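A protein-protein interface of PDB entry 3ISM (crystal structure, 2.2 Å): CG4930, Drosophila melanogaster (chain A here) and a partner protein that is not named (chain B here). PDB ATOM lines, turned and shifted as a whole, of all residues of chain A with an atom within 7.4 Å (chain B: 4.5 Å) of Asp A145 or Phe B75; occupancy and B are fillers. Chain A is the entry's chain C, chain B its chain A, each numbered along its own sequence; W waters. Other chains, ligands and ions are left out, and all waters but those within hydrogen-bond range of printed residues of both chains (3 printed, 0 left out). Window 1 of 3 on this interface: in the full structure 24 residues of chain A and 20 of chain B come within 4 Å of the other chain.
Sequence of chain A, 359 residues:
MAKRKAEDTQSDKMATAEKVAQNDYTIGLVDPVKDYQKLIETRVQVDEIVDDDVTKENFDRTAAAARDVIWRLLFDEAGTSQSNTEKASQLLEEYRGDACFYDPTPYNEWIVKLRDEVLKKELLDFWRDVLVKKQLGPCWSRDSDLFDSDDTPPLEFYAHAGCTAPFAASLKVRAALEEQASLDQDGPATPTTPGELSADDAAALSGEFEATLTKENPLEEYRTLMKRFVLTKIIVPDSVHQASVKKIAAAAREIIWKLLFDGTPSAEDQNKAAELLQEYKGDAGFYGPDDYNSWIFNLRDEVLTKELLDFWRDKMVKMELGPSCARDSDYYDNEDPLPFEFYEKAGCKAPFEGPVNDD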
ATOM      1  N   ASP A  52     -20.493  -0.784  16.632  1.00  0.00           N
ATOM      2  CA  ASP A  52     -20.206   0.656  16.613  1.00  0.00           C
ATOM      3  C   ASP A  52     -20.032   1.210  18.023  1.00  0.00           C
ATOM      4  O   ASP A  52     -19.268   2.149  18.207  1.00  0.00           O
ATOM      5  CB  ASP A  52     -21.293   1.457  15.874  1.00  0.00           C
ATOM      6  CG  ASP A  52     -21.448   1.044  14.421  1.00  0.00           C
ATOM      7  OD1 ASP A  52     -20.637   1.450  13.560  1.00  0.00           O
ATOM      8  OD2 ASP A  52     -22.417   0.319  14.145  1.00  0.00           O
ATOM      9  N   CYS A 100     -13.475  15.491  13.857  1.00  0.00           N
ATOM     10  CA  CYS A 100     -14.421  15.980  12.847  1.00  0.00           C
ATOM     11  C   CYS A 100     -15.249  14.854  12.230  1.00  0.00           C
ATOM     12  O   CYS A 100     -16.354  15.095  11.739  1.00  0.00           O
ATOM     13  CB  CYS A 100     -13.687  16.677  11.694  1.00  0.00           C
ATOM     14  SG  CYS A 100     -12.924  18.268  12.056  1.00  0.00           S
ATOM     15  N   PHE A 101     -14.685  13.651  12.190  1.00  0.00           N
ATOM     16  CA  PHE A 101     -15.344  12.494  11.599  1.00  0.00           C
ATOM     17  C   PHE A 101     -16.051  11.652  12.670  1.00  0.00           C
ATOM     18  O   PHE A 101     -17.214  11.267  12.500  1.00  0.00           O
ATOM     19  CB  PHE A 101     -14.324  11.638  10.828  1.00  0.00           C
ATOM     20  CG  PHE A 101     -14.925  10.419  10.160  1.00  0.00           C
ATOM     21  CD1 PHE A 101     -15.532  10.518   8.910  1.00  0.00           C
ATOM     22  CD2 PHE A 101     -14.883   9.174  10.778  1.00  0.00           C
ATOM     23  CE1 PHE A 101     -16.083   9.400   8.292  1.00  0.00           C
ATOM     24  CE2 PHE A 101     -15.441   8.044  10.160  1.00  0.00           C
ATOM     25  CZ  PHE A 101     -16.040   8.160   8.921  1.00  0.00           C
ATOM     26  N   TYR A 102     -15.341  11.361  13.762  1.00  0.00           N
ATOM     27  CA  TYR A 102     -15.868  10.469  14.813  1.00  0.00           C
ATOM     28  C   TYR A 102     -16.712  11.144  15.913  1.00  0.00           C
ATOM     29  O   TYR A 102     -17.714  10.575  16.326  1.00  0.00           O
ATOM     30  CB  TYR A 102     -14.749   9.678  15.497  1.00  0.00           C
ATOM     31  CG  TYR A 102     -13.945   8.784  14.596  1.00  0.00           C
ATOM     32  CD1 TYR A 102     -12.653   9.136  14.227  1.00  0.00           C
ATOM     33  CD2 TYR A 102     -14.468   7.587  14.120  1.00  0.00           C
ATOM     34  CE1 TYR A 102     -11.897   8.339  13.405  1.00  0.00           C
ATOM     35  CE2 TYR A 102     -13.725   6.776  13.283  1.00  0.00           C
ATOM     36  CZ  TYR A 102     -12.435   7.157  12.938  1.00  0.00           C
ATOM     37  OH  TYR A 102     -11.680   6.360  12.128  1.00  0.00           O
ATOM     38  N   PRO A 104     -17.188  15.253  17.148  1.00  0.00           N
ATOM     39  CA  PRO A 104     -16.842  16.667  17.288  1.00  0.00           C
ATOM     40  C   PRO A 104     -17.258  17.314  18.605  1.00  0.00           C
ATOM     41  O   PRO A 104     -16.593  18.244  19.046  1.00  0.00           O
ATOM     42  CB  PRO A 104     -17.585  17.335  16.111  1.00  0.00           C
ATOM     43  CG  PRO A 104     -17.985  16.220  15.215  1.00  0.00           C
ATOM     44  CD  PRO A 104     -18.202  15.049  16.102  1.00  0.00           C
ATOM     45  N   TRP A 140     -16.960  22.359  12.380  1.00  0.00           N
ATOM     46  CA  TRP A 140     -18.176  22.926  11.782  1.00  0.00           C
ATOM     47  C   TRP A 140     -18.325  22.508  10.312  1.00  0.00           C
ATOM     48  O   TRP A 140     -17.615  21.615   9.859  1.00  0.00           O
ATOM     49  CB  TRP A 140     -18.219  24.459  11.937  1.00  0.00           C
ATOM     50  CG  TRP A 140     -17.202  25.259  11.175  1.00  0.00           C
ATOM     51  CD1 TRP A 140     -15.847  25.223  11.327  1.00  0.00           C
ATOM     52  CD2 TRP A 140     -17.467  26.280  10.197  1.00  0.00           C
ATOM     53  NE1 TRP A 140     -15.249  26.140  10.488  1.00  0.00           N
ATOM     54  CE2 TRP A 140     -16.223  26.809   9.794  1.00  0.00           C
ATOM     55  CE3 TRP A 140     -18.638  26.790   9.615  1.00  0.00           C
ATOM     56  CZ2 TRP A 140     -16.113  27.818   8.823  1.00  0.00           C
ATOM     57  CZ3 TRP A 140     -18.533  27.780   8.658  1.00  0.00           C
ATOM     58  CH2 TRP A 140     -17.278  28.288   8.270  1.00  0.00           C
ATOM     59  N   SER A 141     -19.214  23.152   9.554  1.00  0.00           N
ATOM     60  CA  SER A 141     -19.467  22.670   8.183  1.00  0.00           C
ATOM     61  C   SER A 141     -18.291  22.807   7.203  1.00  0.00           C
ATOM     62  O   SER A 141     -18.295  22.199   6.133  1.00  0.00           O
ATOM     63  CB  SER A 141     -20.756  23.258   7.591  1.00  0.00           C
ATOM     64  OG  SER A 141     -20.666  24.657   7.462  1.00  0.00           O
ATOM     65  N   ARG A 142     -17.286  23.594   7.568  1.00  0.00           N
ATOM     66  CA  ARG A 142     -16.112  23.730   6.719  1.00  0.00           C
ATOM     67  C   ARG A 142     -15.319  22.428   6.719  1.00  0.00           C
ATOM     68  O   ARG A 142     -14.735  22.058   5.701  1.00  0.00           O
ATOM     69  CB  ARG A 142     -15.242  24.896   7.193  1.00  0.00           C
ATOM     70  CG  ARG A 142     -14.156  25.364   6.231  1.00  0.00           C
ATOM     71  CD  ARG A 142     -14.698  25.914   4.926  1.00  0.00           C
ATOM     72  NE  ARG A 142     -15.676  26.992   5.078  1.00  0.00           N
ATOM     73  CZ  ARG A 142     -15.384  28.291   5.067  1.00  0.00           C
ATOM     74  NH1 ARG A 142     -14.123  28.700   4.931  1.00  0.00           N
ATOM     75  NH2 ARG A 142     -16.356  29.185   5.199  1.00  0.00           N
ATOM     76  N   ASP A 143     -15.327  21.730   7.849  1.00  0.00           N
ATOM     77  CA  ASP A 143     -14.452  20.575   8.027  1.00  0.00           C
ATOM     78  C   ASP A 143     -15.122  19.265   8.465  1.00  0.00           C
ATOM     79  O   ASP A 143     -14.434  18.259   8.647  1.00  0.00           O
ATOM     80  CB  ASP A 143     -13.312  20.967   9.001  1.00  0.00           C
ATOM     81  CG  ASP A 143     -13.813  21.804  10.193  1.00  0.00           C
ATOM     82  OD1 ASP A 143     -14.865  21.451  10.770  1.00  0.00           O
ATOM     83  OD2 ASP A 143     -13.157  22.808  10.555  1.00  0.00           O
ATOM     84  N   SER A 144     -16.440  19.245   8.636  1.00  0.00           N
ATOM     85  CA  SER A 144     -17.078  18.030   9.180  1.00  0.00           C
ATOM     86  C   SER A 144     -18.425  17.695   8.521  1.00  0.00           C
ATOM     87  O   SER A 144     -19.251  18.583   8.336  1.00  0.00           O
ATOM     88  CB  SER A 144     -17.244  18.175  10.696  1.00  0.00           C
ATOM     89  OG  SER A 144     -18.002  17.121  11.267  1.00  0.00           O
ATOM     90  N   ASP A 145     -18.651  16.426   8.170  1.00  0.00           N
ATOM     91  CA  ASP A 145     -19.956  16.036   7.599  1.00  0.00           C
ATOM     92  C   ASP A 145     -21.079  15.936   8.647  1.00  0.00           C
ATOM     93  O   ASP A 145     -22.224  15.602   8.328  1.00  0.00           O
ATOM     94  CB  ASP A 145     -19.884  14.784   6.691  1.00  0.00           C
ATOM     95  CG  ASP A 145     -19.505  13.492   7.432  1.00  0.00           C
ATOM     96  OD1 ASP A 145     -19.299  13.491   8.668  1.00  0.00           O
ATOM     97  OD2 ASP A 145     -19.410  12.451   6.740  1.00  0.00           O
ATOM     98  N   LEU A 146     -20.740  16.246   9.889  1.00  0.00           N
ATOM     99  CA  LEU A 146     -21.719  16.301  10.970  1.00  0.00           C
ATOM    100  C   LEU A 146     -22.423  17.646  11.032  1.00  0.00           C
ATOM    101  O   LEU A 146     -23.328  17.838  11.842  1.00  0.00           O
ATOM    102  CB  LEU A 146     -21.055  16.000  12.311  1.00  0.00           C
ATOM    103  CG  LEU A 146     -20.782  14.510  12.496  1.00  0.00           C
ATOM    104  CD1 LEU A 146     -19.387  14.097  12.028  1.00  0.00           C
ATOM    105  CD2 LEU A 146     -20.969  14.167  13.926  1.00  0.00           C
ATOM    106  N   PHE A 147     -22.002  18.573  10.164  1.00  0.00           N
ATOM    107  CA  PHE A 147     -22.537  19.923  10.139  1.00  0.00           C
ATOM    108  C   PHE A 147     -22.925  20.330   8.705  1.00  0.00           C
ATOM    109  O   PHE A 147     -22.526  19.686   7.721  1.00  0.00           O
ATOM    110  CB  PHE A 147     -21.501  20.924  10.692  1.00  0.00           C
ATOM    111  CG  PHE A 147     -21.029  20.640  12.112  1.00  0.00           C
ATOM    112  CD1 PHE A 147     -19.995  19.738  12.359  1.00  0.00           C
ATOM    113  CD2 PHE A 147     -21.585  21.327  13.195  1.00  0.00           C
ATOM    114  CE1 PHE A 147     -19.538  19.487  13.677  1.00  0.00           C
ATOM    115  CE2 PHE A 147     -21.135  21.099  14.503  1.00  0.00           C
ATOM    116  CZ  PHE A 147     -20.104  20.171  14.746  1.00  0.00           C
ATOM    117  N   ASP A 148     -23.717  21.396   8.596  1.00  0.00           N
ATOM    118  CA  ASP A 148     -24.110  21.957   7.293  1.00  0.00           C
ATOM    119  C   ASP A 148     -24.224  23.493   7.372  1.00  0.00           C
ATOM    120  O   ASP A 148     -23.967  24.085   8.424  1.00  0.00           O
ATOM    121  CB  ASP A 148     -25.406  21.327   6.764  1.00  0.00           C
ATOM    122  CG  ASP A 148     -26.627  21.621   7.656  1.00  0.00           C
ATOM    123  OD1 ASP A 148     -27.467  20.707   7.808  1.00  0.00           O
ATOM    124  OD2 ASP A 148     -26.749  22.741   8.202  1.00  0.00           O
ATOM    125  N   CYS B  73     -27.034  12.370  17.633  1.00  0.00           N
ATOM    126  CA  CYS B  73     -27.073  11.264  16.689  1.00  0.00           C
ATOM    127  C   CYS B  73     -25.713  10.831  16.182  1.00  0.00           C
ATOM    128  O   CYS B  73     -24.825  11.660  15.927  1.00  0.00           O
ATOM    129  CB  CYS B  73     -27.909  11.632  15.487  1.00  0.00           C
ATOM    130  SG  CYS B  73     -29.492  12.261  15.928  1.00  0.00           S
ATOM    131  N   ASP B  74     -25.586   9.520  16.008  1.00  0.00           N
ATOM    132  CA  ASP B  74     -24.351   8.884  15.585  1.00  0.00           C
ATOM    133  C   ASP B  74     -24.564   8.153  14.273  1.00  0.00           C
ATOM    134  O   ASP B  74     -25.555   7.444  14.113  1.00  0.00           O
ATOM    135  CB  ASP B  74     -23.907   7.868  16.646  1.00  0.00           C
ATOM    136  CG  ASP B  74     -23.789   8.489  18.025  1.00  0.00           C
ATOM    137  OD1 ASP B  74     -23.628   9.728  18.106  1.00  0.00           O
ATOM    138  OD2 ASP B  74     -23.861   7.752  19.031  1.00  0.00           O
ATOM    139  N   PHE B  75     -23.624   8.325  13.354  1.00  0.00           N
ATOM    140  CA  PHE B  75     -23.542   7.497  12.169  1.00  0.00           C
ATOM    141  C   PHE B  75     -23.235   6.063  12.567  1.00  0.00           C
ATOM    142  O   PHE B  75     -22.239   5.812  13.250  1.00  0.00           O
ATOM    143  CB  PHE B  75     -22.436   8.010  11.269  1.00  0.00           C
ATOM    144  CG  PHE B  75     -22.796   9.255  10.508  1.00  0.00           C
ATOM    145  CD1 PHE B  75     -23.697   9.204   9.460  1.00  0.00           C
ATOM    146  CD2 PHE B  75     -22.216  10.484  10.834  1.00  0.00           C
ATOM    147  CE1 PHE B  75     -24.001  10.356   8.726  1.00  0.00           C
ATOM    148  CE2 PHE B  75     -22.531  11.634  10.109  1.00  0.00           C
ATOM    149  CZ  PHE B  75     -23.418  11.562   9.055  1.00  0.00           C
ATOM    150  N   LYS B  76     -24.101   5.130  12.187  1.00  0.00           N
ATOM    151  CA  LYS B  76     -23.919   3.729  12.577  1.00  0.00           C
ATOM    152  C   LYS B  76     -24.288   2.743  11.481  1.00  0.00           C
ATOM    153  O   LYS B  76     -25.183   3.003  10.672  1.00  0.00           O
ATOM    154  CB  LYS B  76     -24.676   3.403  13.870  1.00  0.00           C
ATOM    155  CG  LYS B  76     -26.174   3.676  13.845  1.00  0.00           C
ATOM    156  CD  LYS B  76     -26.719   3.851  15.275  1.00  0.00           C
ATOM    157  CE  LYS B  76     -28.152   4.410  15.261  1.00  0.00           C
ATOM    158  NZ  LYS B  76     -28.291   5.622  14.364  1.00  0.00           N
ATOM    159  N   ASN B  89     -18.383   3.029   8.486  1.00  0.00           N
ATOM    160  CA  ASN B  89     -17.649   4.290   8.642  1.00  0.00           C
ATOM    161  C   ASN B  89     -16.222   4.271   8.063  1.00  0.00           C
ATOM    162  O   ASN B  89     -15.785   5.266   7.465  1.00  0.00           O
ATOM    163  CB  ASN B  89     -17.631   4.719  10.118  1.00  0.00           C
ATOM    164  CG  ASN B  89     -18.971   5.302  10.554  1.00  0.00           C
ATOM    165  OD1 ASN B  89     -19.626   5.988   9.780  1.00  0.00           O
ATOM    166  ND2 ASN B  89     -19.388   5.008  11.776  1.00  0.00           N
ATOM    167  N   ASP B  98     -18.333  12.894   2.070  1.00  0.00           N
ATOM    168  CA  ASP B  98     -19.205  12.913   3.227  1.00  0.00           C
ATOM    169  C   ASP B  98     -20.110  11.680   3.237  1.00  0.00           C
ATOM    170  O   ASP B  98     -20.413  11.115   2.187  1.00  0.00           O
ATOM    171  CB  ASP B  98     -20.096  14.171   3.187  1.00  0.00           C
ATOM    172  CG  ASP B  98     -19.357  15.417   3.615  1.00  0.00           C
ATOM    173  OD1 ASP B  98     -18.113  15.369   3.710  1.00  0.00           O
ATOM    174  OD2 ASP B  98     -20.020  16.452   3.887  1.00  0.00           O
ATOM    175  N   ARG B  99     -20.530  11.268   4.432  1.00  0.00           N
ATOM    176  CA  ARG B  99     -21.663  10.363   4.576  1.00  0.00           C
ATOM    177  C   ARG B  99     -22.916  11.211   4.344  1.00  0.00           C
ATOM    178  O   ARG B  99     -23.311  12.000   5.206  1.00  0.00           O
ATOM    179  CB  ARG B  99     -21.671   9.747   5.988  1.00  0.00           C
ATOM    180  CG  ARG B  99     -20.500   8.826   6.248  1.00  0.00           C
ATOM    181  CD  ARG B  99     -20.213   8.623   7.718  1.00  0.00           C
ATOM    182  NE  ARG B  99     -19.732   9.840   8.371  1.00  0.00           N
ATOM    183  CZ  ARG B  99     -19.228   9.848   9.595  1.00  0.00           C
ATOM    184  NH1 ARG B  99     -19.131   8.704  10.252  1.00  0.00           N
ATOM    185  NH2 ARG B  99     -18.817  10.985  10.151  1.00  0.00           N
ATOM    186  N   HIS B 101     -26.766  11.829   3.779  1.00  0.00           N
ATOM    187  CA  HIS B 101     -28.147  11.406   4.017  1.00  0.00           C
ATOM    188  C   HIS B 101     -28.948  11.477   2.735  1.00  0.00           C
ATOM    189  O   HIS B 101     -28.921  12.507   2.044  1.00  0.00           O
ATOM    190  CB  HIS B 101     -28.859  12.383   4.968  1.00  0.00           C
ATOM    191  CG  HIS B 101     -28.467  12.262   6.401  1.00  0.00           C
ATOM    192  ND1 HIS B 101     -27.289  12.773   6.893  1.00  0.00           N
ATOM    193  CD2 HIS B 101     -29.132  11.753   7.465  1.00  0.00           C
ATOM    194  CE1 HIS B 101     -27.226  12.549   8.191  1.00  0.00           C
ATOM    195  NE2 HIS B 101     -28.328  11.924   8.561  1.00  0.00           N
ATOM    196  N   PHE B 119     -29.507   8.254  10.602  1.00  0.00           N
ATOM    197  CA  PHE B 119     -28.046   8.131  10.702  1.00  0.00           C
ATOM    198  C   PHE B 119     -27.519   6.687  10.480  1.00  0.00           C
ATOM    199  O   PHE B 119     -26.316   6.429  10.595  1.00  0.00           O
ATOM    200  CB  PHE B 119     -27.536   8.748  12.023  1.00  0.00           C
ATOM    201  CG  PHE B 119     -27.490  10.267  12.015  1.00  0.00           C
ATOM    202  CD1 PHE B 119     -26.297  10.944  11.736  1.00  0.00           C
ATOM    203  CD2 PHE B 119     -28.636  11.018  12.273  1.00  0.00           C
ATOM    204  CE1 PHE B 119     -26.241  12.358  11.720  1.00  0.00           C
ATOM    205  CE2 PHE B 119     -28.596  12.444  12.264  1.00  0.00           C
ATOM    206  CZ  PHE B 119     -27.397  13.107  11.992  1.00  0.00           C
ATOM    207  N   LEU B 121     -26.076   3.983   8.237  1.00  0.00           N
ATOM    208  CA  LEU B 121     -25.231   4.109   7.052  1.00  0.00           C
ATOM    209  C   LEU B 121     -25.930   3.569   5.810  1.00  0.00           C
ATOM    210  O   LEU B 121     -25.527   3.874   4.687  1.00  0.00           O
ATOM    211  CB  LEU B 121     -23.884   3.422   7.271  1.00  0.00           C
ATOM    212  CG  LEU B 121     -22.989   4.108   8.325  1.00  0.00           C
ATOM    213  CD1 LEU B 121     -21.807   3.229   8.635  1.00  0.00           C
ATOM    214  CD2 LEU B 121     -22.530   5.492   7.847  1.00  0.00           C
ATOM    215  N   MET B 124     -27.073   6.342   3.662  1.00  0.00           N
ATOM    216  CA  MET B 124     -25.986   7.189   3.163  1.00  0.00           C
ATOM    217  C   MET B 124     -25.485   6.839   1.767  1.00  0.00           C
ATOM    218  O   MET B 124     -25.392   5.665   1.403  1.00  0.00           O
ATOM    219  CB  MET B 124     -24.777   7.144   4.140  1.00  0.00           C
ATOM    220  CG  MET B 124     -25.129   7.501   5.565  1.00  0.00           C
ATOM    221  SD  MET B 124     -25.728   9.189   5.757  1.00  0.00           S
ATOM    222  CE  MET B 124     -26.823   8.901   7.144  1.00  0.00           C
ATOM    223  N   ASN B 133     -22.994  18.433  -0.344  1.00  0.00           N
ATOM    224  CA  ASN B 133     -23.701  17.958   0.863  1.00  0.00           C
ATOM    225  C   ASN B 133     -24.000  19.058   1.898  1.00  0.00           C
ATOM    226  O   ASN B 133     -25.141  19.253   2.323  1.00  0.00           O
ATOM    227  CB  ASN B 133     -22.902  16.851   1.559  1.00  0.00           C
ATOM    228  CG  ASN B 133     -23.585  16.356   2.802  1.00  0.00           C
ATOM    229  OD1 ASN B 133     -24.820  16.200   2.831  1.00  0.00           O
ATOM    230  ND2 ASN B 133     -22.811  16.117   3.845  1.00  0.00           N
ATOM    231  N   ARG B 134     -22.959  19.792   2.267  1.00  0.00           N
ATOM    232  CA  ARG B 134     -23.032  20.784   3.329  1.00  0.00           C
ATOM    233  C   ARG B 134     -23.637  22.113   2.867  1.00  0.00           C
ATOM    234  O   ARG B 134     -23.977  22.983   3.681  1.00  0.00           O
ATOM    235  CB  ARG B 134     -21.626  20.988   3.883  1.00  0.00           C
ATOM    236  CG  ARG B 134     -21.013  19.678   4.398  1.00  0.00           C
ATOM    237  CD  ARG B 134     -19.611  19.898   4.905  1.00  0.00           C
ATOM    238  NE  ARG B 134     -18.767  18.716   4.760  1.00  0.00           N
ATOM    239  CZ  ARG B 134     -17.448  18.721   4.899  1.00  0.00           C
ATOM    240  NH1 ARG B 134     -16.769  17.587   4.727  1.00  0.00           N
ATOM    241  NH2 ARG B 134     -16.805  19.847   5.207  1.00  0.00           N
HETATM  242  O   HOH W   1     -23.389  14.392   6.195  1.00  0.00           O
HETATM  243  O   HOH W   2     -19.045   1.396  10.846  1.00  0.00           O
HETATM  244  O   HOH W   3     -23.716  17.542   6.719  1.00  0.00           O
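The guanidinium group (NH2) of Arg B99 lies within hydrogen-bond range of the backbone carbonyl oxygen (O) of Phe A101 (2.9 Å). NH2 of Arg B99 is in salt-bridge range of OD1 of Asp A145. The backbone carbonyl oxygen of Ser A141 lies close to the guanidinium group of Arg B134, 2.9 Å away. NH2 of Arg B134 is in hydrogen-bond range of O of Arg A142 (3.1 Å).
The backbone carbonyl oxygen (O) of Lys B76 sits at hydrogen-bond distance from the backbone NH (N) of Leu B121 (2.8 Å). The side-chain amide oxygen (OD1) of Asn B89 sits at hydrogen-bond distance from the guanidinium group (NH1) of Arg B99, at 2.8 Å. The guanidinium group of Arg B134 is in salt-bridge range of the side-chain carboxylate of Asp B98, 2.7 Å away. SG of Cys A100 sits close to O of Asp A143, 3.7 Å away. The side-chain hydroxyl (OG) of Ser A144 is in hydrogen-bond range of the backbone carbonyl oxygen (O) of Cys A100 (2.7 Å). The backbone carbonyl oxygen (O) of Asp A148 sits close to the side-chain hydroxyl (OG) of Ser A141 (3.5 Å).
Among the printed residues, pairs that only touch across the chains: Asp A145 with Asp B98, Phe A101 with Asn B89, Ser A144 with Arg B134, Asp A143 with Arg B134, Phe A147 with Arg B134, Leu A146 with Arg B99, Asp A148 with Arg B134, Asp A52 with Lys B76 and Asp A145 with Phe B75.
Cys A100 touches none of the printed residues of chain B. Of the printed residues of chain B, Phe A101 touches Asn B89 (3.2 Å) and Arg B99 (2.9 Å). Of the printed residues of chain B, Arg A142 touches Arg B134. Printed residues of chain B within 4 Å of Asp A145: Phe B75, Asp B98 and Arg B99. Cys B73 touches none of the printed residues of chain A. Of the printed residues of chain A, Phe B75 touches Asp A145. Of the printed residues of chain A, Arg B99 touches Phe A101 (2.9 Å), Asp A145 (2.8 Å) and Leu A146 (3.7 Å). The nearest printed residue of chain A that does not touch Phe B75 is Leu A146 (4.1 Å). The nearest printed residue of chain B that does not touch Asp A52 is Asn B89 (4.2 Å).
Printed residues of chain B that touch a printed residue of chain A: Phe B75, Lys B76, Asn B89, Asp B98, Arg B99 and Arg B134. Hydrophobic or aromatic side chains of chain B that line the printed part of chain A: Phe B75. Printed residues of chain A that touch a printed residue of chain B: Asp A52, Phe A101, Ser A141, Arg A142, Asp A143, Ser A144, Asp A145, Leu A146, Phe A147 and Asp A148. Among the printed residues, 13 pairs touch across the chains.
Water W1 lies within hydrogen-bond range of the backbone carbonyl oxygen of Arg B99 (2.6 Å), the backbone carbonyl oxygen of Asp A145 (2.7 Å) and the side-chain amide nitrogen of Asn B133 (3.0 Å). Water W3 lies within hydrogen-bond range of the backbone carbonyl oxygen (O) of Phe A147 (2.6 Å), the backbone carbonyl oxygen (O) of Asp A145 (2.9 Å) and the side-chain amide nitrogen (ND2) of Asn B133 (3.3 Å). Water W2 lies within hydrogen-bond range of the backbone NH (N) of Asn B89 and the side-chain carboxylate (OD1) of Asp A52.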
